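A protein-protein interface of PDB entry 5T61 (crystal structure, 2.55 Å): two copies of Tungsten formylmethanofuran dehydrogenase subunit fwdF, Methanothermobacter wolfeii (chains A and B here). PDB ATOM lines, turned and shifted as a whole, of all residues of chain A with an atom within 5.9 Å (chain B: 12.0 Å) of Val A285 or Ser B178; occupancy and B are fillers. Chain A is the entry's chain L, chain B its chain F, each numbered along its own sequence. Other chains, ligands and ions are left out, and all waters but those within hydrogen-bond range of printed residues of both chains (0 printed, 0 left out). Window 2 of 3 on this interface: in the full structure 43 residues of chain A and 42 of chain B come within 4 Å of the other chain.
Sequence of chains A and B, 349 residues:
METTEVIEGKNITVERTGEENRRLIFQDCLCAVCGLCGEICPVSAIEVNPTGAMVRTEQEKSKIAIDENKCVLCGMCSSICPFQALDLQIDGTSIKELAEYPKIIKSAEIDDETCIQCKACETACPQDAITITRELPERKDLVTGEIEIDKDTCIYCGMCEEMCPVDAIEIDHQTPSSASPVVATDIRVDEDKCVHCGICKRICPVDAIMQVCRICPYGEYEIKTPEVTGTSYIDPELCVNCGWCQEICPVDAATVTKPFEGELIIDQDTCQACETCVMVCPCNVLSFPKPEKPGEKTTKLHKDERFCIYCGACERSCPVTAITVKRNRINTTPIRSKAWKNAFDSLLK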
ATOM      1  N   TRP A 244      25.842  18.083  17.268  1.00  0.00           N
ATOM      2  CA  TRP A 244      27.087  17.680  16.612  1.00  0.00           C
ATOM      3  C   TRP A 244      28.110  17.175  17.622  1.00  0.00           C
ATOM      4  O   TRP A 244      28.793  16.172  17.377  1.00  0.00           O
ATOM      5  CB  TRP A 244      27.671  18.859  15.832  1.00  0.00           C
ATOM      6  CG  TRP A 244      27.173  18.987  14.424  1.00  0.00           C
ATOM      7  CD1 TRP A 244      26.241  19.867  13.973  1.00  0.00           C
ATOM      8  CD2 TRP A 244      27.580  18.228  13.283  1.00  0.00           C
ATOM      9  NE1 TRP A 244      26.029  19.709  12.636  1.00  0.00           N
ATOM     10  CE2 TRP A 244      26.843  18.707  12.182  1.00  0.00           C
ATOM     11  CE3 TRP A 244      28.492  17.191  13.082  1.00  0.00           C
ATOM     12  CZ2 TRP A 244      26.986  18.186  10.905  1.00  0.00           C
ATOM     13  CZ3 TRP A 244      28.634  16.675  11.808  1.00  0.00           C
ATOM     14  CH2 TRP A 244      27.885  17.173  10.736  1.00  0.00           C
ATOM     15  N   LEU A 264      12.495  16.324   7.959  1.00  0.00           N
ATOM     16  CA  LEU A 264      12.997  17.035   6.795  1.00  0.00           C
ATOM     17  C   LEU A 264      12.586  16.251   5.556  1.00  0.00           C
ATOM     18  O   LEU A 264      12.726  15.023   5.525  1.00  0.00           O
ATOM     19  CB  LEU A 264      14.518  17.151   6.857  1.00  0.00           C
ATOM     20  CG  LEU A 264      15.153  18.459   7.314  1.00  0.00           C
ATOM     21  CD1 LEU A 264      16.650  18.399   7.062  1.00  0.00           C
ATOM     22  CD2 LEU A 264      14.533  19.632   6.586  1.00  0.00           C
ATOM     23  N   CYS A 281      21.667  26.867   6.704  1.00  0.00           N
ATOM     24  CA  CYS A 281      21.510  25.928   7.811  1.00  0.00           C
ATOM     25  C   CYS A 281      22.434  26.263   8.973  1.00  0.00           C
ATOM     26  O   CYS A 281      23.659  26.134   8.858  1.00  0.00           O
ATOM     27  CB  CYS A 281      21.779  24.498   7.351  1.00  0.00           C
ATOM     28  SG  CYS A 281      21.982  23.346   8.722  1.00  0.00           S
ATOM     29  N   CYS A 283      22.754  24.599  11.708  1.00  0.00           N
ATOM     30  CA  CYS A 283      23.194  23.377  12.369  1.00  0.00           C
ATOM     31  C   CYS A 283      24.051  22.484  11.476  1.00  0.00           C
ATOM     32  O   CYS A 283      24.417  21.379  11.894  1.00  0.00           O
ATOM     33  CB  CYS A 283      21.981  22.587  12.874  1.00  0.00           C
ATOM     34  SG  CYS A 283      20.953  23.475  14.069  1.00  0.00           S
ATOM     35  N   ASN A 284      24.366  22.934  10.259  1.00  0.00           N
ATOM     36  CA  ASN A 284      25.186  22.188   9.300  1.00  0.00           C
ATOM     37  C   ASN A 284      24.554  20.831   8.986  1.00  0.00           C
ATOM     38  O   ASN A 284      25.228  19.799   8.949  1.00  0.00           O
ATOM     39  CB  ASN A 284      26.631  22.022   9.779  1.00  0.00           C
ATOM     40  CG  ASN A 284      27.466  23.279   9.569  1.00  0.00           C
ATOM     41  OD1 ASN A 284      27.103  24.165   8.793  1.00  0.00           O
ATOM     42  ND2 ASN A 284      28.629  23.325  10.209  1.00  0.00           N
ATOM     43  N   VAL A 285      23.241  20.833   8.760  1.00  0.00           N
ATOM     44  CA  VAL A 285      22.528  19.598   8.452  1.00  0.00           C
ATOM     45  C   VAL A 285      22.714  19.220   6.988  1.00  0.00           C
ATOM     46  O   VAL A 285      22.712  18.034   6.640  1.00  0.00           O
ATOM     47  CB  VAL A 285      21.035  19.743   8.805  1.00  0.00           C
ATOM     48  CG1 VAL A 285      20.264  18.467   8.467  1.00  0.00           C
ATOM     49  CG2 VAL A 285      20.862  20.109  10.270  1.00  0.00           C
ATOM     50  N   LEU A 286      22.871  20.207   6.113  1.00  0.00           N
ATOM     51  CA  LEU A 286      22.764  20.029   4.676  1.00  0.00           C
ATOM     52  C   LEU A 286      24.145  20.112   4.040  1.00  0.00           C
ATOM     53  O   LEU A 286      24.972  20.938   4.441  1.00  0.00           O
ATOM     54  CB  LEU A 286      21.850  21.116   4.109  1.00  0.00           C
ATOM     55  CG  LEU A 286      20.549  21.188   4.925  1.00  0.00           C
ATOM     56  CD1 LEU A 286      19.735  22.451   4.633  1.00  0.00           C
ATOM     57  CD2 LEU A 286      19.703  19.913   4.751  1.00  0.00           C
ATOM     58  N   SER A 287      24.398  19.274   3.038  1.00  0.00           N
ATOM     59  CA  SER A 287      25.709  19.282   2.407  1.00  0.00           C
ATOM     60  C   SER A 287      25.604  18.798   0.969  1.00  0.00           C
ATOM     61  O   SER A 287      24.619  18.171   0.566  1.00  0.00           O
ATOM     62  CB  SER A 287      26.712  18.421   3.186  1.00  0.00           C
ATOM     63  OG  SER A 287      26.294  17.069   3.225  1.00  0.00           O
ATOM     64  N   HIS A 302      22.226  16.343   0.419  1.00  0.00           N
ATOM     65  CA  HIS A 302      22.288  15.339   1.472  1.00  0.00           C
ATOM     66  C   HIS A 302      21.949  15.974   2.812  1.00  0.00           C
ATOM     67  O   HIS A 302      22.428  17.065   3.134  1.00  0.00           O
ATOM     68  CB  HIS A 302      23.676  14.697   1.543  1.00  0.00           C
ATOM     69  CG  HIS A 302      23.775  13.583   2.541  1.00  0.00           C
ATOM     70  ND1 HIS A 302      24.299  13.759   3.804  1.00  0.00           N
ATOM     71  CD2 HIS A 302      23.427  12.277   2.458  1.00  0.00           C
ATOM     72  CE1 HIS A 302      24.264  12.611   4.457  1.00  0.00           C
ATOM     73  NE2 HIS A 302      23.740  11.695   3.662  1.00  0.00           N
ATOM     74  N   LYS A 303      21.123  15.283   3.587  1.00  0.00           N
ATOM     75  CA  LYS A 303      20.758  15.719   4.924  1.00  0.00           C
ATOM     76  C   LYS A 303      21.184  14.664   5.935  1.00  0.00           C
ATOM     77  O   LYS A 303      21.397  13.495   5.598  1.00  0.00           O
ATOM     78  CB  LYS A 303      19.251  15.930   5.062  1.00  0.00           C
ATOM     79  CG  LYS A 303      18.517  14.608   4.977  1.00  0.00           C
ATOM     80  CD  LYS A 303      17.034  14.719   5.219  1.00  0.00           C
ATOM     81  CE  LYS A 303      16.419  13.334   5.125  1.00  0.00           C
ATOM     82  NZ  LYS A 303      15.112  13.232   5.822  1.00  0.00           N
ATOM     83  N   ASP A 304      21.294  15.089   7.189  1.00  0.00           N
ATOM     84  CA  ASP A 304      21.418  14.169   8.317  1.00  0.00           C
ATOM     85  C   ASP A 304      20.595  14.788   9.440  1.00  0.00           C
ATOM     86  O   ASP A 304      21.072  15.684  10.143  1.00  0.00           O
ATOM     87  CB  ASP A 304      22.875  13.965   8.717  1.00  0.00           C
ATOM     88  CG  ASP A 304      23.060  12.827   9.707  1.00  0.00           C
ATOM     89  OD1 ASP A 304      22.086  12.456  10.399  1.00  0.00           O
ATOM     90  OD2 ASP A 304      24.189  12.298   9.790  1.00  0.00           O
ATOM     91  N   GLU A 305      19.363  14.304   9.615  1.00  0.00           N
ATOM     92  CA  GLU A 305      18.452  14.949  10.552  1.00  0.00           C
ATOM     93  C   GLU A 305      18.887  14.808  12.002  1.00  0.00           C
ATOM     94  O   GLU A 305      18.256  15.418  12.870  1.00  0.00           O
ATOM     95  CB  GLU A 305      17.039  14.379  10.432  1.00  0.00           C
ATOM     96  CG  GLU A 305      16.299  14.716   9.155  1.00  0.00           C
ATOM     97  CD  GLU A 305      14.807  14.467   9.283  1.00  0.00           C
ATOM     98  OE1 GLU A 305      14.316  14.426  10.432  1.00  0.00           O
ATOM     99  OE2 GLU A 305      14.137  14.257   8.248  1.00  0.00           O
ATOM    100  N   ARG A 306      19.925  14.011  12.288  1.00  0.00           N
ATOM    101  CA  ARG A 306      20.433  13.937  13.656  1.00  0.00           C
ATOM    102  C   ARG A 306      20.829  15.308  14.179  1.00  0.00           C
ATOM    103  O   ARG A 306      20.719  15.569  15.381  1.00  0.00           O
ATOM    104  CB  ARG A 306      21.632  12.995  13.746  1.00  0.00           C
ATOM    105  CG  ARG A 306      21.308  11.520  13.655  1.00  0.00           C
ATOM    106  CD  ARG A 306      22.600  10.726  13.659  1.00  0.00           C
ATOM    107  NE  ARG A 306      23.511  11.110  12.585  1.00  0.00           N
ATOM    108  CZ  ARG A 306      24.814  10.845  12.606  1.00  0.00           C
ATOM    109  NH1 ARG A 306      25.336  10.214  13.649  1.00  0.00           N
ATOM    110  NH2 ARG A 306      25.598  11.213  11.600  1.00  0.00           N
ATOM    111  N   PHE A 307      21.285  16.192  13.299  1.00  0.00           N
ATOM    112  CA  PHE A 307      21.745  17.520  13.673  1.00  0.00           C
ATOM    113  C   PHE A 307      20.667  18.571  13.474  1.00  0.00           C
ATOM    114  O   PHE A 307      20.916  19.757  13.698  1.00  0.00           O
ATOM    115  CB  PHE A 307      22.988  17.882  12.857  1.00  0.00           C
ATOM    116  CG  PHE A 307      24.012  16.787  12.816  1.00  0.00           C
ATOM    117  CD1 PHE A 307      24.607  16.337  13.982  1.00  0.00           C
ATOM    118  CD2 PHE A 307      24.355  16.185  11.617  1.00  0.00           C
ATOM    119  CE1 PHE A 307      25.545  15.324  13.954  1.00  0.00           C
ATOM    120  CE2 PHE A 307      25.296  15.167  11.581  1.00  0.00           C
ATOM    121  CZ  PHE A 307      25.891  14.737  12.750  1.00  0.00           C
ATOM    122  N   CYS A 308      19.476  18.154  13.073  1.00  0.00           N
ATOM    123  CA  CYS A 308      18.408  19.067  12.714  1.00  0.00           C
ATOM    124  C   CYS A 308      17.602  19.515  13.930  1.00  0.00           C
ATOM    125  O   CYS A 308      17.346  18.728  14.847  1.00  0.00           O
ATOM    126  CB  CYS A 308      17.506  18.376  11.697  1.00  0.00           C
ATOM    127  SG  CYS A 308      16.032  19.262  11.317  1.00  0.00           S
ATOM    128  N   ILE A 309      17.196  20.788  13.936  1.00  0.00           N
ATOM    129  CA  ILE A 309      16.338  21.328  14.984  1.00  0.00           C
ATOM    130  C   ILE A 309      15.005  21.832  14.453  1.00  0.00           C
ATOM    131  O   ILE A 309      14.199  22.348  15.235  1.00  0.00           O
ATOM    132  CB  ILE A 309      17.037  22.448  15.785  1.00  0.00           C
ATOM    133  CG1 ILE A 309      17.248  23.690  14.912  1.00  0.00           C
ATOM    134  CG2 ILE A 309      18.333  21.944  16.413  1.00  0.00           C
ATOM    135  CD1 ILE A 309      17.748  24.894  15.674  1.00  0.00           C
ATOM    136  N   GLN B 174      39.503  19.339   8.772  1.00  0.00           N
ATOM    137  CA  GLN B 174      38.392  19.902   8.016  1.00  0.00           C
ATOM    138  C   GLN B 174      37.277  20.260   8.987  1.00  0.00           C
ATOM    139  O   GLN B 174      37.219  19.748  10.108  1.00  0.00           O
ATOM    140  CB  GLN B 174      37.862  18.929   6.958  1.00  0.00           C
ATOM    141  CG  GLN B 174      37.279  17.655   7.556  1.00  0.00           C
ATOM    142  CD  GLN B 174      36.526  16.814   6.544  1.00  0.00           C
ATOM    143  OE1 GLN B 174      35.513  16.192   6.871  1.00  0.00           O
ATOM    144  NE2 GLN B 174      37.011  16.795   5.310  1.00  0.00           N
ATOM    145  N   THR B 175      36.376  21.124   8.528  1.00  0.00           N
ATOM    146  CA  THR B 175      35.111  21.349   9.222  1.00  0.00           C
ATOM    147  C   THR B 175      34.112  20.269   8.818  1.00  0.00           C
ATOM    148  O   THR B 175      33.971  19.980   7.625  1.00  0.00           O
ATOM    149  CB  THR B 175      34.558  22.735   8.900  1.00  0.00           C
ATOM    150  OG1 THR B 175      35.594  23.710   9.066  1.00  0.00           O
ATOM    151  CG2 THR B 175      33.407  23.087   9.837  1.00  0.00           C
ATOM    152  N   PRO B 176      33.413  19.651   9.768  1.00  0.00           N
ATOM    153  CA  PRO B 176      32.482  18.576   9.405  1.00  0.00           C
ATOM    154  C   PRO B 176      31.314  19.069   8.565  1.00  0.00           C
ATOM    155  O   PRO B 176      30.916  20.235   8.615  1.00  0.00           O
ATOM    156  CB  PRO B 176      31.994  18.049  10.761  1.00  0.00           C
ATOM    157  CG  PRO B 176      32.992  18.526  11.760  1.00  0.00           C
ATOM    158  CD  PRO B 176      33.536  19.815  11.226  1.00  0.00           C
ATOM    159  N   SER B 177      30.776  18.147   7.774  1.00  0.00           N
ATOM    160  CA  SER B 177      29.532  18.314   7.044  1.00  0.00           C
ATOM    161  C   SER B 177      28.701  17.056   7.249  1.00  0.00           C
ATOM    162  O   SER B 177      29.197  16.035   7.731  1.00  0.00           O
ATOM    163  CB  SER B 177      29.778  18.555   5.549  1.00  0.00           C
ATOM    164  OG  SER B 177      30.229  17.367   4.922  1.00  0.00           O
ATOM    165  N   SER B 178      27.417  17.131   6.896  1.00  0.00           N
ATOM    166  CA  SER B 178      26.579  15.943   7.023  1.00  0.00           C
ATOM    167  C   SER B 178      27.065  14.823   6.112  1.00  0.00           C
ATOM    168  O   SER B 178      26.844  13.643   6.408  1.00  0.00           O
ATOM    169  CB  SER B 178      25.121  16.273   6.718  1.00  0.00           C
ATOM    170  OG  SER B 178      24.974  16.900   5.455  1.00  0.00           O
ATOM    171  N   ALA B 179      27.717  15.170   4.997  1.00  0.00           N
ATOM    172  CA  ALA B 179      28.276  14.150   4.116  1.00  0.00           C
ATOM    173  C   ALA B 179      29.544  13.535   4.699  1.00  0.00           C
ATOM    174  O   ALA B 179      29.777  12.329   4.549  1.00  0.00           O
ATOM    175  CB  ALA B 179      28.556  14.744   2.736  1.00  0.00           C
ATOM    176  N   SER B 180      30.374  14.339   5.367  1.00  0.00           N
ATOM    177  CA  SER B 180      31.649  13.885   5.928  1.00  0.00           C
ATOM    178  C   SER B 180      31.724  14.304   7.390  1.00  0.00           C
ATOM    179  O   SER B 180      32.423  15.266   7.740  1.00  0.00           O
ATOM    180  CB  SER B 180      32.830  14.443   5.131  1.00  0.00           C
ATOM    181  OG  SER B 180      34.068  14.011   5.669  1.00  0.00           O
ATOM    182  N   PRO B 181      31.020  13.557   8.309  1.00  0.00           N
ATOM    183  CA  PRO B 181      30.913  13.984   9.717  1.00  0.00           C
ATOM    184  C   PRO B 181      32.153  13.629  10.533  1.00  0.00           C
ATOM    185  O   PRO B 181      32.101  12.895  11.524  1.00  0.00           O
ATOM    186  CB  PRO B 181      29.661  13.231  10.187  1.00  0.00           C
ATOM    187  CG  PRO B 181      29.713  11.952   9.406  1.00  0.00           C
ATOM    188  CD  PRO B 181      30.236  12.336   8.040  1.00  0.00           C
ATOM    189  N   VAL B 182      33.294  14.179  10.121  1.00  0.00           N
ATOM    190  CA  VAL B 182      34.569  13.936  10.783  1.00  0.00           C
ATOM    191  C   VAL B 182      35.341  15.246  10.818  1.00  0.00           C
ATOM    192  O   VAL B 182      35.151  16.122   9.969  1.00  0.00           O
ATOM    193  CB  VAL B 182      35.393  12.832  10.072  1.00  0.00           C
ATOM    194  CG1 VAL B 182      34.695  11.482  10.171  1.00  0.00           C
ATOM    195  CG2 VAL B 182      35.628  13.204   8.614  1.00  0.00           C
ATOM    196  N   VAL B 183      36.215  15.383  11.822  1.00  0.00           N
ATOM    197  CA  VAL B 183      37.024  16.593  11.958  1.00  0.00           C
ATOM    198  C   VAL B 183      38.345  16.487  11.222  1.00  0.00           C
ATOM    199  O   VAL B 183      39.120  17.454  11.213  1.00  0.00           O
ATOM    200  CB  VAL B 183      37.342  16.924  13.430  1.00  0.00           C
ATOM    201  CG1 VAL B 183      36.064  17.079  14.244  1.00  0.00           C
ATOM    202  CG2 VAL B 183      38.275  15.872  14.022  1.00  0.00           C
ATOM    203  N   ALA B 184      38.633  15.339  10.617  1.00  0.00           N
ATOM    204  CA  ALA B 184      39.842  15.143   9.834  1.00  0.00           C
ATOM    205  C   ALA B 184      39.666  13.884   9.002  1.00  0.00           C
ATOM    206  O   ALA B 184      38.929  12.971   9.388  1.00  0.00           O
ATOM    207  CB  ALA B 184      41.083  15.028  10.726  1.00  0.00           C
ATOM    208  N   THR B 185      40.346  13.846   7.857  1.00  0.00           N
ATOM    209  CA  THR B 185      40.220  12.730   6.933  1.00  0.00           C
ATOM    210  C   THR B 185      41.461  11.852   6.842  1.00  0.00           C
ATOM    211  O   THR B 185      41.383  10.776   6.239  1.00  0.00           O
ATOM    212  CB  THR B 185      39.852  13.238   5.530  1.00  0.00           C
ATOM    213  OG1 THR B 185      40.815  14.206   5.094  1.00  0.00           O
ATOM    214  CG2 THR B 185      38.471  13.869   5.545  1.00  0.00           C
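The backbone NH (N) of Ser B180 lies within hydrogen-bond range of the side-chain hydroxyl (OG) of Ser B177 (3.1 Å).
NE1 of Trp A244 sits at hydrogen-bond distance from O of Cys A283, at 2.4 Å.
SG of Cys A281 sits close to N of Val A285 (2.8 Å).
The backbone NH (N) of Asp A304 sits at hydrogen-bond distance from the backbone carbonyl oxygen (O) of Val A285 (3.3 Å).
N of Ser A287 sits at hydrogen-bond distance from O of His A302 (3.0 Å).
NH2 of Arg A306 lies within salt-bridge range of OD2 of Asp A304 (2.5 Å).
OG of Ser B178 is in hydrogen-bond range of O of Val A285 (2.8 Å).
The side-chain hydroxyl (OG) of Ser B178 sits at hydrogen-bond distance from the side-chain hydroxyl (OG) of Ser A287 (2.6 Å).
OG of Ser B178 is in hydrogen-bond range of O of His A302 (3.4 Å).
N of Ala B179 is in hydrogen-bond range of OG of Ser A287 (3.0 Å).
No position is printed for both chains.
CB of Pro B176 touches CZ3 of Trp A244, 3.8 Å away.
O of Ser B177 touches CH2 of Trp A244, at 3.5 Å.
Trp A244 touches Ser B178.
Trp A244 touches Pro B181.
Ser B178 touches Leu A286.
Ser A287 touches Ser B177 (CB to CB, 3.9 Å).
N of Ala B179 touches ND1 of His A302, 3.9 Å away.
Asp A304 touches Ser B178.
Of the 12 printed residues of chain B, 5 touch a printed residue of chain A.
Hydrophobic or aromatic side chains of chain B within 4 Å of the printed part of chain A: Pro B176, Ala B179 and Pro B181.
Hydrophobic or aromatic side chains of chain A within 4 Å of the printed part of chain B: Trp A244 and His A302.
Among the printed residues, 12 pairs touch across the chains.
Among the printed residues, no Asp or Glu carboxylate lies within 4 Å of a Lys or Arg side-chain nitrogen of the other chain.
Of chain B, only Ser B178 comes within 4 Å of Val A285.
No residue of chain B comes within 4 Å of Cys A283.
Leu A286 touches one residue of chain B.
Ser A287 touches just these residues of chain B: Ser B177, Ser B178 and Ala B179.
Of the printed residues of chain B, Asp A304 touches Ser B178 (3.8 Å).
No residue of chain B comes within 4 Å of Phe A307.
No residue of chain B comes within 4 Å of Cys A308.
Of the printed residues of chain A, Pro B176 touches Trp A244.
Printed residues of chain A within 4 Å of Pro B181: Trp A244.
Printed residues of chain A within 4 Å of Ser B177: Trp A244 (3.5 Å) and Ser A287 (3.9 Å).
Printed residues of chain B within 4 Å of Trp A244: Pro B176 (3.8 Å), Ser B177 (3.5 Å), Ser B178 (3.9 Å) and Pro B181 (3.9 Å).
Of the printed residues of chain A, Ala B179 touches Ser A287 (3.0 Å) and His A302 (3.9 Å).
Leu A264 touches none of the printed residues of chain B.
Ser B180 touches none of the printed residues of chain A.
The nearest residue of chain B that does not touch Val A285 is Ala B179 (6.0 Å).
The nearest printed residue of chain A that does not touch Ser B178 is Asn A284 (4.02 Å).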
